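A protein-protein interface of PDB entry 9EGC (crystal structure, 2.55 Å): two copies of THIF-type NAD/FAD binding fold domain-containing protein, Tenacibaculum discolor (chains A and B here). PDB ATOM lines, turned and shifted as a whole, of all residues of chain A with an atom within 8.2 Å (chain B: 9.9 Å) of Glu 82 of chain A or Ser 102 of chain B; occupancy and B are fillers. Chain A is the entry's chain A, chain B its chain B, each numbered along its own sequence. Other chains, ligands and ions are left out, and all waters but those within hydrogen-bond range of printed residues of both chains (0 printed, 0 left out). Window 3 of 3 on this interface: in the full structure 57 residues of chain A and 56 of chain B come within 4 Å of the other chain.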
ATOM      1  N   VAL A  70       3.204  -0.887  17.776  1.00  0.00           N
ATOM      2  CA  VAL A  70       2.000  -1.512  17.232  1.00  0.00           C
ATOM      3  C   VAL A  70       2.421  -2.759  16.469  1.00  0.00           C
ATOM      4  O   VAL A  70       3.295  -2.708  15.596  1.00  0.00           O
ATOM      5  CB  VAL A  70       1.226  -0.538  16.325  1.00  0.00           C
ATOM      6  CG1 VAL A  70       0.085  -1.260  15.643  1.00  0.00           C
ATOM      7  CG2 VAL A  70       0.697   0.642  17.125  1.00  0.00           C
ATOM      8  N   GLU A  71       1.805  -3.880  16.813  1.00  0.00           N
ATOM      9  CA  GLU A  71       2.040  -5.191  16.235  1.00  0.00           C
ATOM     10  C   GLU A  71       0.796  -5.677  15.498  1.00  0.00           C
ATOM     11  O   GLU A  71      -0.317  -5.200  15.735  1.00  0.00           O
ATOM     12  CB  GLU A  71       2.478  -6.138  17.367  1.00  0.00           C
ATOM     13  CG  GLU A  71       2.615  -7.608  17.070  1.00  0.00           C
ATOM     14  CD  GLU A  71       3.162  -8.350  18.277  1.00  0.00           C
ATOM     15  OE1 GLU A  71       2.551  -9.372  18.680  1.00  0.00           O
ATOM     16  OE2 GLU A  71       4.118  -7.829  18.897  1.00  0.00           O
ATOM     17  N   ASN A  72       1.000  -6.625  14.581  1.00  0.00           N
ATOM     18  CA  ASN A  72      -0.112  -7.159  13.795  1.00  0.00           C
ATOM     19  C   ASN A  72      -1.210  -7.733  14.678  1.00  0.00           C
ATOM     20  O   ASN A  72      -2.400  -7.483  14.449  1.00  0.00           O
ATOM     21  CB  ASN A  72       0.393  -8.223  12.828  1.00  0.00           C
ATOM     22  CG  ASN A  72       0.469  -7.726  11.422  1.00  0.00           C
ATOM     23  OD1 ASN A  72      -0.515  -7.766  10.690  1.00  0.00           O
ATOM     24  ND2 ASN A  72       1.629  -7.224  11.035  1.00  0.00           N
ATOM     25  N   LEU A  75      -4.403  -5.905  15.977  1.00  0.00           N
ATOM     26  CA  LEU A  75      -5.465  -5.384  15.135  1.00  0.00           C
ATOM     27  C   LEU A  75      -6.815  -6.031  15.396  1.00  0.00           C
ATOM     28  O   LEU A  75      -7.837  -5.438  15.044  1.00  0.00           O
ATOM     29  CB  LEU A  75      -5.084  -5.543  13.676  1.00  0.00           C
ATOM     30  CG  LEU A  75      -3.798  -4.801  13.326  1.00  0.00           C
ATOM     31  CD1 LEU A  75      -3.457  -5.068  11.876  1.00  0.00           C
ATOM     32  CD2 LEU A  75      -3.962  -3.309  13.595  1.00  0.00           C
ATOM     33  N   TYR A  80      -5.757   0.524  16.325  1.00  0.00           N
ATOM     34  CA  TYR A  80      -4.674   0.777  15.372  1.00  0.00           C
ATOM     35  C   TYR A  80      -5.031   0.236  13.992  1.00  0.00           C
ATOM     36  O   TYR A  80      -5.931  -0.593  13.835  1.00  0.00           O
ATOM     37  CB  TYR A  80      -3.323   0.192  15.851  1.00  0.00           C
ATOM     38  CG  TYR A  80      -2.987   0.694  17.225  1.00  0.00           C
ATOM     39  CD1 TYR A  80      -2.592   2.012  17.420  1.00  0.00           C
ATOM     40  CD2 TYR A  80      -3.108  -0.127  18.339  1.00  0.00           C
ATOM     41  CE1 TYR A  80      -2.333   2.494  18.687  1.00  0.00           C
ATOM     42  CE2 TYR A  80      -2.845   0.349  19.612  1.00  0.00           C
ATOM     43  CZ  TYR A  80      -2.465   1.660  19.773  1.00  0.00           C
ATOM     44  OH  TYR A  80      -2.202   2.145  21.019  1.00  0.00           O
ATOM     45  N   THR A  81      -4.289   0.715  12.994  1.00  0.00           N
ATOM     46  CA  THR A  81      -4.474   0.419  11.578  1.00  0.00           C
ATOM     47  C   THR A  81      -3.251  -0.292  11.005  1.00  0.00           C
ATOM     48  O   THR A  81      -2.189  -0.342  11.623  1.00  0.00           O
ATOM     49  CB  THR A  81      -4.693   1.709  10.793  1.00  0.00           C
ATOM     50  OG1 THR A  81      -3.503   2.501  10.894  1.00  0.00           O
ATOM     51  CG2 THR A  81      -5.858   2.494  11.349  1.00  0.00           C
ATOM     52  N   GLU A  82      -3.386  -0.803   9.774  1.00  0.00           N
ATOM     53  CA  GLU A  82      -2.250  -1.449   9.118  1.00  0.00           C
ATOM     54  C   GLU A  82      -1.058  -0.502   8.999  1.00  0.00           C
ATOM     55  O   GLU A  82       0.099  -0.938   9.061  1.00  0.00           O
ATOM     56  CB  GLU A  82      -2.648  -1.973   7.738  1.00  0.00           C
ATOM     57  CG  GLU A  82      -3.639  -3.146   7.731  1.00  0.00           C
ATOM     58  CD  GLU A  82      -3.856  -3.709   6.321  1.00  0.00           C
ATOM     59  OE1 GLU A  82      -4.526  -4.758   6.178  1.00  0.00           O
ATOM     60  OE2 GLU A  82      -3.354  -3.086   5.355  1.00  0.00           O
ATOM     61  N   GLY A  83      -1.318   0.793   8.799  1.00  0.00           N
ATOM     62  CA  GLY A  83      -0.244   1.766   8.705  1.00  0.00           C
ATOM     63  C   GLY A  83       0.470   2.028  10.014  1.00  0.00           C
ATOM     64  O   GLY A  83       1.622   2.483   9.999  1.00  0.00           O
ATOM     65  N   ASP A  84      -0.177   1.721  11.145  1.00  0.00           N
ATOM     66  CA  ASP A  84       0.406   1.934  12.461  1.00  0.00           C
ATOM     67  C   ASP A  84       1.422   0.865  12.835  1.00  0.00           C
ATOM     68  O   ASP A  84       2.228   1.091  13.739  1.00  0.00           O
ATOM     69  CB  ASP A  84      -0.699   1.964  13.537  1.00  0.00           C
ATOM     70  CG  ASP A  84      -1.624   3.172  13.418  1.00  0.00           C
ATOM     71  OD1 ASP A  84      -1.136   4.229  12.984  1.00  0.00           O
ATOM     72  OD2 ASP A  84      -2.836   3.072  13.745  1.00  0.00           O
ATOM     73  N   VAL A  85       1.430  -0.274  12.142  1.00  0.00           N
ATOM     74  CA  VAL A  85       2.259  -1.392  12.569  1.00  0.00           C
ATOM     75  C   VAL A  85       3.722  -0.991  12.510  1.00  0.00           C
ATOM     76  O   VAL A  85       4.179  -0.411  11.518  1.00  0.00           O
ATOM     77  CB  VAL A  85       1.959  -2.630  11.713  1.00  0.00           C
ATOM     78  CG1 VAL A  85       2.929  -3.734  12.011  1.00  0.00           C
ATOM     79  CG2 VAL A  85       0.542  -3.115  11.992  1.00  0.00           C
ATOM     80  N   SER A  86       4.454  -1.281  13.592  1.00  0.00           N
ATOM     81  CA  SER A  86       5.860  -0.962  13.868  1.00  0.00           C
ATOM     82  C   SER A  86       6.049   0.432  14.455  1.00  0.00           C
ATOM     83  O   SER A  86       7.166   0.776  14.794  1.00  0.00           O
ATOM     84  CB  SER A  86       6.761  -1.057  12.628  1.00  0.00           C
ATOM     85  OG  SER A  86       6.722  -2.350  12.058  1.00  0.00           O
ATOM     86  N   VAL A  87       5.004   1.203  14.655  1.00  0.00           N
ATOM     87  CA  VAL A  87       5.107   2.541  15.219  1.00  0.00           C
ATOM     88  C   VAL A  87       4.796   2.469  16.703  1.00  0.00           C
ATOM     89  O   VAL A  87       4.071   1.581  17.157  1.00  0.00           O
ATOM     90  CB  VAL A  87       4.141   3.492  14.484  1.00  0.00           C
ATOM     91  CG1 VAL A  87       4.274   4.914  14.979  1.00  0.00           C
ATOM     92  CG2 VAL A  87       4.379   3.405  12.996  1.00  0.00           C
ATOM     93  N   LYS B  16      -5.070 -15.740  10.660  1.00  0.00           N
ATOM     94  CA  LYS B  16      -3.876 -14.986  10.294  1.00  0.00           C
ATOM     95  C   LYS B  16      -3.296 -14.415  11.584  1.00  0.00           C
ATOM     96  O   LYS B  16      -3.968 -14.389  12.618  1.00  0.00           O
ATOM     97  CB  LYS B  16      -4.191 -13.865   9.280  1.00  0.00           C
ATOM     98  CG  LYS B  16      -2.974 -13.121   8.725  1.00  0.00           C
ATOM     99  CD  LYS B  16      -3.385 -11.951   7.837  1.00  0.00           C
ATOM    100  CE  LYS B  16      -2.178 -11.099   7.466  1.00  0.00           C
ATOM    101  NZ  LYS B  16      -1.508 -10.558   8.687  1.00  0.00           N
ATOM    102  N   ARG B  18      -2.980 -11.546  12.299  1.00  0.00           N
ATOM    103  CA  ARG B  18      -3.908 -10.486  12.684  1.00  0.00           C
ATOM    104  C   ARG B  18      -4.992 -11.004  13.626  1.00  0.00           C
ATOM    105  O   ARG B  18      -5.430 -10.287  14.536  1.00  0.00           O
ATOM    106  CB  ARG B  18      -4.527  -9.892  11.418  1.00  0.00           C
ATOM    107  CG  ARG B  18      -5.909  -9.299  11.583  1.00  0.00           C
ATOM    108  CD  ARG B  18      -6.610  -9.136  10.230  1.00  0.00           C
ATOM    109  NE  ARG B  18      -5.925  -8.240   9.295  1.00  0.00           N
ATOM    110  CZ  ARG B  18      -6.063  -6.917   9.299  1.00  0.00           C
ATOM    111  NH1 ARG B  18      -6.850  -6.331  10.199  1.00  0.00           N
ATOM    112  NH2 ARG B  18      -5.423  -6.176   8.407  1.00  0.00           N
ATOM    113  N   TYR B  19      -5.447 -12.246  13.422  1.00  0.00           N
ATOM    114  CA  TYR B  19      -6.440 -12.883  14.282  1.00  0.00           C
ATOM    115  C   TYR B  19      -5.804 -13.856  15.270  1.00  0.00           C
ATOM    116  O   TYR B  19      -6.479 -14.762  15.775  1.00  0.00           O
ATOM    117  CB  TYR B  19      -7.514 -13.596  13.452  1.00  0.00           C
ATOM    118  CG  TYR B  19      -8.243 -12.680  12.494  1.00  0.00           C
ATOM    119  CD1 TYR B  19      -8.955 -11.583  12.970  1.00  0.00           C
ATOM    120  CD2 TYR B  19      -8.215 -12.906  11.122  1.00  0.00           C
ATOM    121  CE1 TYR B  19      -9.609 -10.737  12.112  1.00  0.00           C
ATOM    122  CE2 TYR B  19      -8.863 -12.058  10.251  1.00  0.00           C
ATOM    123  CZ  TYR B  19      -9.562 -10.974  10.745  1.00  0.00           C
ATOM    124  OH  TYR B  19     -10.210 -10.118   9.881  1.00  0.00           O
ATOM    125  N   LYS B  35     -15.143 -14.790   7.709  1.00  0.00           N
ATOM    126  CA  LYS B  35     -14.390 -13.962   6.771  1.00  0.00           C
ATOM    127  C   LYS B  35     -15.246 -13.525   5.587  1.00  0.00           C
ATOM    128  O   LYS B  35     -15.199 -12.357   5.187  1.00  0.00           O
ATOM    129  CB  LYS B  35     -13.148 -14.709   6.289  1.00  0.00           C
ATOM    130  CG  LYS B  35     -12.281 -13.923   5.309  1.00  0.00           C
ATOM    131  CD  LYS B  35     -10.994 -14.662   5.018  1.00  0.00           C
ATOM    132  CE  LYS B  35     -10.118 -13.913   4.025  1.00  0.00           C
ATOM    133  NZ  LYS B  35     -10.589 -14.085   2.617  1.00  0.00           N
ATOM    134  N   LEU B  55     -15.424  -5.984  12.016  1.00  0.00           N
ATOM    135  CA  LEU B  55     -14.304  -6.219  11.100  1.00  0.00           C
ATOM    136  C   LEU B  55     -13.083  -6.752  11.842  1.00  0.00           C
ATOM    137  O   LEU B  55     -12.457  -7.728  11.411  1.00  0.00           O
ATOM    138  CB  LEU B  55     -13.939  -4.938  10.358  1.00  0.00           C
ATOM    139  CG  LEU B  55     -12.672  -5.016   9.498  1.00  0.00           C
ATOM    140  CD1 LEU B  55     -12.839  -6.044   8.384  1.00  0.00           C
ATOM    141  CD2 LEU B  55     -12.256  -3.652   8.929  1.00  0.00           C
ATOM    142  N   ARG B  56     -12.720  -6.106  12.957  1.00  0.00           N
ATOM    143  CA  ARG B  56     -11.547  -6.542  13.708  1.00  0.00           C
ATOM    144  C   ARG B  56     -11.720  -7.959  14.228  1.00  0.00           C
ATOM    145  O   ARG B  56     -10.744  -8.709  14.312  1.00  0.00           O
ATOM    146  CB  ARG B  56     -11.255  -5.573  14.852  1.00  0.00           C
ATOM    147  CG  ARG B  56     -10.857  -4.166  14.383  1.00  0.00           C
ATOM    148  CD  ARG B  56     -10.394  -3.340  15.573  1.00  0.00           C
ATOM    149  NE  ARG B  56     -10.024  -1.974  15.225  1.00  0.00           N
ATOM    150  CZ  ARG B  56      -8.840  -1.641  14.717  1.00  0.00           C
ATOM    151  NH1 ARG B  56      -7.928  -2.574  14.485  1.00  0.00           N
ATOM    152  NH2 ARG B  56      -8.554  -0.376  14.443  1.00  0.00           N
ATOM    153  N   GLU B  60     -15.200  -9.900   7.279  1.00  0.00           N
ATOM    154  CA  GLU B  60     -14.551  -9.103   6.250  1.00  0.00           C
ATOM    155  C   GLU B  60     -15.435  -8.818   5.035  1.00  0.00           C
ATOM    156  O   GLU B  60     -14.976  -8.163   4.094  1.00  0.00           O
ATOM    157  CB  GLU B  60     -13.266  -9.806   5.805  1.00  0.00           C
ATOM    158  CG  GLU B  60     -12.182  -9.788   6.878  1.00  0.00           C
ATOM    159  CD  GLU B  60     -10.897 -10.462   6.448  1.00  0.00           C
ATOM    160  OE1 GLU B  60     -10.716 -10.757   5.238  1.00  0.00           O
ATOM    161  OE2 GLU B  60     -10.067 -10.703   7.348  1.00  0.00           O
ATOM    162  N   LYS B  94     -15.656   3.500   4.945  1.00  0.00           N
ATOM    163  CA  LYS B  94     -14.875   2.574   4.119  1.00  0.00           C
ATOM    164  C   LYS B  94     -13.388   2.895   4.190  1.00  0.00           C
ATOM    165  O   LYS B  94     -12.549   1.985   4.229  1.00  0.00           O
ATOM    166  CB  LYS B  94     -15.358   2.593   2.665  1.00  0.00           C
ATOM    167  CG  LYS B  94     -14.588   1.645   1.737  1.00  0.00           C
ATOM    168  CD  LYS B  94     -15.184   1.652   0.334  1.00  0.00           C
ATOM    169  CE  LYS B  94     -14.371   0.839  -0.702  1.00  0.00           C
ATOM    170  NZ  LYS B  94     -14.216  -0.621  -0.420  1.00  0.00           N
ATOM    171  N   ALA B  95     -13.037   4.180   4.205  1.00  0.00           N
ATOM    172  CA  ALA B  95     -11.637   4.543   4.406  1.00  0.00           C
ATOM    173  C   ALA B  95     -11.138   4.021   5.746  1.00  0.00           C
ATOM    174  O   ALA B  95     -10.119   3.324   5.815  1.00  0.00           O
ATOM    175  CB  ALA B  95     -11.468   6.056   4.317  1.00  0.00           C
ATOM    176  N   ARG B  96     -11.892   4.290   6.813  1.00  0.00           N
ATOM    177  CA  ARG B  96     -11.515   3.820   8.141  1.00  0.00           C
ATOM    178  C   ARG B  96     -11.369   2.303   8.170  1.00  0.00           C
ATOM    179  O   ARG B  96     -10.345   1.775   8.620  1.00  0.00           O
ATOM    180  CB  ARG B  96     -12.553   4.292   9.160  1.00  0.00           C
ATOM    181  CG  ARG B  96     -12.408   3.684  10.516  1.00  0.00           C
ATOM    182  CD  ARG B  96     -11.156   4.140  11.218  1.00  0.00           C
ATOM    183  NE  ARG B  96     -11.060   3.513  12.536  1.00  0.00           N
ATOM    184  CZ  ARG B  96      -9.992   3.567  13.326  1.00  0.00           C
ATOM    185  NH1 ARG B  96      -8.910   4.229  12.952  1.00  0.00           N
ATOM    186  NH2 ARG B  96     -10.014   2.959  14.499  1.00  0.00           N
ATOM    187  N   LEU B  97     -12.375   1.585   7.659  1.00  0.00           N
ATOM    188  CA  LEU B  97     -12.349   0.124   7.706  1.00  0.00           C
ATOM    189  C   LEU B  97     -11.209  -0.448   6.870  1.00  0.00           C
ATOM    190  O   LEU B  97     -10.512  -1.371   7.310  1.00  0.00           O
ATOM    191  CB  LEU B  97     -13.696  -0.433   7.232  1.00  0.00           C
ATOM    192  CG  LEU B  97     -14.847  -0.123   8.177  1.00  0.00           C
ATOM    193  CD1 LEU B  97     -16.167  -0.497   7.549  1.00  0.00           C
ATOM    194  CD2 LEU B  97     -14.639  -0.864   9.499  1.00  0.00           C
ATOM    195  N   LYS B  98     -10.987   0.098   5.672  1.00  0.00           N
ATOM    196  CA  LYS B  98      -9.970  -0.465   4.794  1.00  0.00           C
ATOM    197  C   LYS B  98      -8.559  -0.137   5.265  1.00  0.00           C
ATOM    198  O   LYS B  98      -7.617  -0.840   4.891  1.00  0.00           O
ATOM    199  CB  LYS B  98     -10.193   0.014   3.359  1.00  0.00           C
ATOM    200  CG  LYS B  98     -11.220  -0.809   2.554  1.00  0.00           C
ATOM    201  CD  LYS B  98     -10.538  -1.926   1.765  1.00  0.00           C
ATOM    202  CE  LYS B  98     -11.294  -2.234   0.492  1.00  0.00           C
ATOM    203  NZ  LYS B  98     -10.453  -2.911  -0.544  1.00  0.00           N
ATOM    204  N   SER B  99      -8.388   0.895   6.091  1.00  0.00           N
ATOM    205  CA  SER B  99      -7.090   1.116   6.713  1.00  0.00           C
ATOM    206  C   SER B  99      -6.820   0.129   7.850  1.00  0.00           C
ATOM    207  O   SER B  99      -5.653  -0.131   8.168  1.00  0.00           O
ATOM    208  CB  SER B  99      -6.983   2.568   7.194  1.00  0.00           C
ATOM    209  OG  SER B  99      -7.722   2.788   8.377  1.00  0.00           O
ATOM    210  N   ILE B 100      -7.873  -0.438   8.450  1.00  0.00           N
ATOM    211  CA  ILE B 100      -7.714  -1.522   9.416  1.00  0.00           C
ATOM    212  C   ILE B 100      -7.404  -2.841   8.712  1.00  0.00           C
ATOM    213  O   ILE B 100      -6.532  -3.601   9.148  1.00  0.00           O
ATOM    214  CB  ILE B 100      -8.974  -1.617  10.296  1.00  0.00           C
ATOM    215  CG1 ILE B 100      -9.116  -0.350  11.145  1.00  0.00           C
ATOM    216  CG2 ILE B 100      -8.984  -2.899  11.128  1.00  0.00           C
ATOM    217  CD1 ILE B 100     -10.448  -0.207  11.811  1.00  0.00           C
ATOM    218  N   ASN B 101      -8.073  -3.122   7.596  1.00  0.00           N
ATOM    219  CA  ASN B 101      -7.866  -4.372   6.858  1.00  0.00           C
ATOM    220  C   ASN B 101      -7.947  -4.043   5.366  1.00  0.00           C
ATOM    221  O   ASN B 101      -9.033  -3.810   4.825  1.00  0.00           O
ATOM    222  CB  ASN B 101      -8.877  -5.438   7.260  1.00  0.00           C
ATOM    223  CG  ASN B 101      -8.471  -6.831   6.803  1.00  0.00           C
ATOM    224  OD1 ASN B 101      -7.726  -6.993   5.834  1.00  0.00           O
ATOM    225  ND2 ASN B 101      -8.980  -7.845   7.489  1.00  0.00           N
ATOM    226  N   SER B 102      -6.784  -3.977   4.717  1.00  0.00           N
ATOM    227  CA  SER B 102      -6.740  -3.627   3.301  1.00  0.00           C
ATOM    228  C   SER B 102      -7.364  -4.705   2.419  1.00  0.00           C
ATOM    229  O   SER B 102      -7.926  -4.382   1.369  1.00  0.00           O
ATOM    230  CB  SER B 102      -5.301  -3.336   2.883  1.00  0.00           C
ATOM    231  OG  SER B 102      -4.439  -4.391   3.266  1.00  0.00           O
ATOM    232  N   LYS B 103      -7.245  -5.979   2.796  1.00  0.00           N
ATOM    233  CA  LYS B 103      -7.834  -7.063   2.014  1.00  0.00           C
ATOM    234  C   LYS B 103      -9.309  -7.306   2.333  1.00  0.00           C
ATOM    235  O   LYS B 103      -9.872  -8.301   1.859  1.00  0.00           O
ATOM    236  CB  LYS B 103      -7.053  -8.375   2.185  1.00  0.00           C
ATOM    237  CG  LYS B 103      -5.696  -8.413   1.469  1.00  0.00           C
ATOM    238  CD  LYS B 103      -4.905  -9.705   1.747  1.00  0.00           C
ATOM    239  CE  LYS B 103      -4.318  -9.774   3.156  1.00  0.00           C
ATOM    240  NZ  LYS B 103      -3.432 -10.965   3.327  1.00  0.00           N
ATOM    241  N   ALA B 104      -9.944  -6.462   3.139  1.00  0.00           N
ATOM    242  CA  ALA B 104     -11.351  -6.665   3.450  1.00  0.00           C
ATOM    243  C   ALA B 104     -12.236  -6.268   2.271  1.00  0.00           C
ATOM    244  O   ALA B 104     -11.888  -5.410   1.452  1.00  0.00           O
ATOM    245  CB  ALA B 104     -11.762  -5.871   4.691  1.00  0.00           C
ATOM    246  N   ASN B 105     -13.404  -6.900   2.206  1.00  0.00           N
ATOM    247  CA  ASN B 105     -14.355  -6.702   1.123  1.00  0.00           C
ATOM    248  C   ASN B 105     -15.460  -5.785   1.648  1.00  0.00           C
ATOM    249  O   ASN B 105     -16.499  -6.231   2.130  1.00  0.00           O
ATOM    250  CB  ASN B 105     -14.884  -8.053   0.668  1.00  0.00           C
ATOM    251  CG  ASN B 105     -15.578  -7.986  -0.659  1.00  0.00           C
ATOM    252  OD1 ASN B 105     -16.202  -6.984  -0.995  1.00  0.00           O
ATOM    253  ND2 ASN B 105     -15.481  -9.063  -1.425  1.00  0.00           N
ATOM    254  N   ILE B 106     -15.210  -4.479   1.578  1.00  0.00           N
ATOM    255  CA  ILE B 106     -16.107  -3.462   2.124  1.00  0.00           C
ATOM    256  C   ILE B 106     -16.779  -2.745   0.955  1.00  0.00           C
ATOM    257  O   ILE B 106     -16.150  -1.923   0.278  1.00  0.00           O
ATOM    258  CB  ILE B 106     -15.358  -2.471   3.034  1.00  0.00           C
ATOM    259  CG1 ILE B 106     -14.510  -3.201   4.101  1.00  0.00           C
ATOM    260  CG2 ILE B 106     -16.332  -1.505   3.685  1.00  0.00           C
ATOM    261  CD1 ILE B 106     -15.280  -4.072   5.063  1.00  0.00           C
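NH2 of Arg 18 of chain B is in hydrogen-bond range of O of Ile 100 of chain B, 2.9 Å away. N of Gly 83 of chain A lies close to OG1 of Thr 81 of chain A. The side-chain carboxylate of Glu 60 of chain B sits at hydrogen-bond distance from the side-chain amide nitrogen of Asn 101 of chain B (3.1 Å). The side-chain hydroxyl of Ser 99 of chain B lies within hydrogen-bond range of the backbone carbonyl oxygen of Arg 96 of chain B. The side-chain carboxylate (OD2) of Asp 84 of chain A sits at hydrogen-bond distance from the backbone NH (N) of Thr 81 of chain A (2.9 Å). The backbone NH (N) of Lys 103 of chain B sits at hydrogen-bond distance from the side-chain amide oxygen (OD1) of Asn 101 of chain B (3.2 Å).
Of the 12 printed residues of chain A, 5 touch a printed residue of chain B. Hydrophobic or aromatic side chains of chain A that line the printed part of chain B: Leu 75. Along chain A the printed residues that touch a printed residue of chain B span positions 72 to 82. Of the 20 printed residues of chain B, 8 touch a printed residue of chain A. Among the printed residues, 12 pairs touch across the chains.
The backbone carbonyl oxygen (O) of Leu 75 of chain A lies within hydrogen-bond range of the guanidinium group (NH1) of Arg 56 of chain B, at 2.9 Å. O of Tyr 80 of chain A sits at hydrogen-bond distance from NH2 of Arg 56 of chain B (2.7 Å). The side-chain carboxylate (OE2) of Glu 82 of chain A sits at hydrogen-bond distance from the side-chain hydroxyl (OG) of Ser 102 of chain B (2.7 Å). The backbone carbonyl oxygen of Ser 99 of chain B is in hydrogen-bond range of the backbone NH of Glu 82 of chain A (2.9 Å). OE1 of Glu 82 of chain A is in salt-bridge range of NH2 of Arg 18 of chain B (2.8 Å).
Among the printed residues, merely in contact across the chains: Asn 72 of chain A with Lys 16 of chain B, Asn 72 of chain A with Arg 18 of chain B, Leu 75 of chain A with Arg 18 of chain B, Thr 81 of chain A with Arg 96 of chain B, Thr 81 of chain A with Ser 99 of chain B, Glu 82 of chain A with Ile 100 of chain B and Glu 82 of chain A with Asn 101 of chain B.
No position is printed for both chains. Of the 12 pairs that touch across the chains among the printed residues, none has its exchanged pair printed and touching as well.
Of chain B, only Arg 18 (2.8 Å), Ser 99 (2.9 Å), Ile 100 (3.3 Å), Asn 101 (3.4 Å) and Ser 102 (2.7 Å) come within 4 Å of Glu 82 of chain A. Of chain A, only Glu 82 comes within 4 Å of Ser 102 of chain B. Of chain B, only Arg 96 and Ser 99 come within 4 Å of Thr 81 of chain A. No residue of chain B comes within 4 Å of Gly 83 of chain A. No residue of chain B comes within 4 Å of Val 85 of chain A. Of the printed residues of chain A, Arg 56 of chain B touches Leu 75 and Tyr 80. Of the printed residues of chain B, Tyr 80 of chain A touches Arg 56 (2.7 Å). Printed residues of chain A within 4 Å of Arg 18 of chain B: Asn 72 (3.8 Å), Leu 75 (3.98 Å) and Glu 82 (2.8 Å). Of the printed residues of chain A, Asn 101 of chain B touches Glu 82. Printed residues of chain A within 4 Å of Arg 96 of chain B: Thr 81. Ser 86 of chain A touches none of the printed residues of chain B. Val 87 of chain A touches none of the printed residues of chain B.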
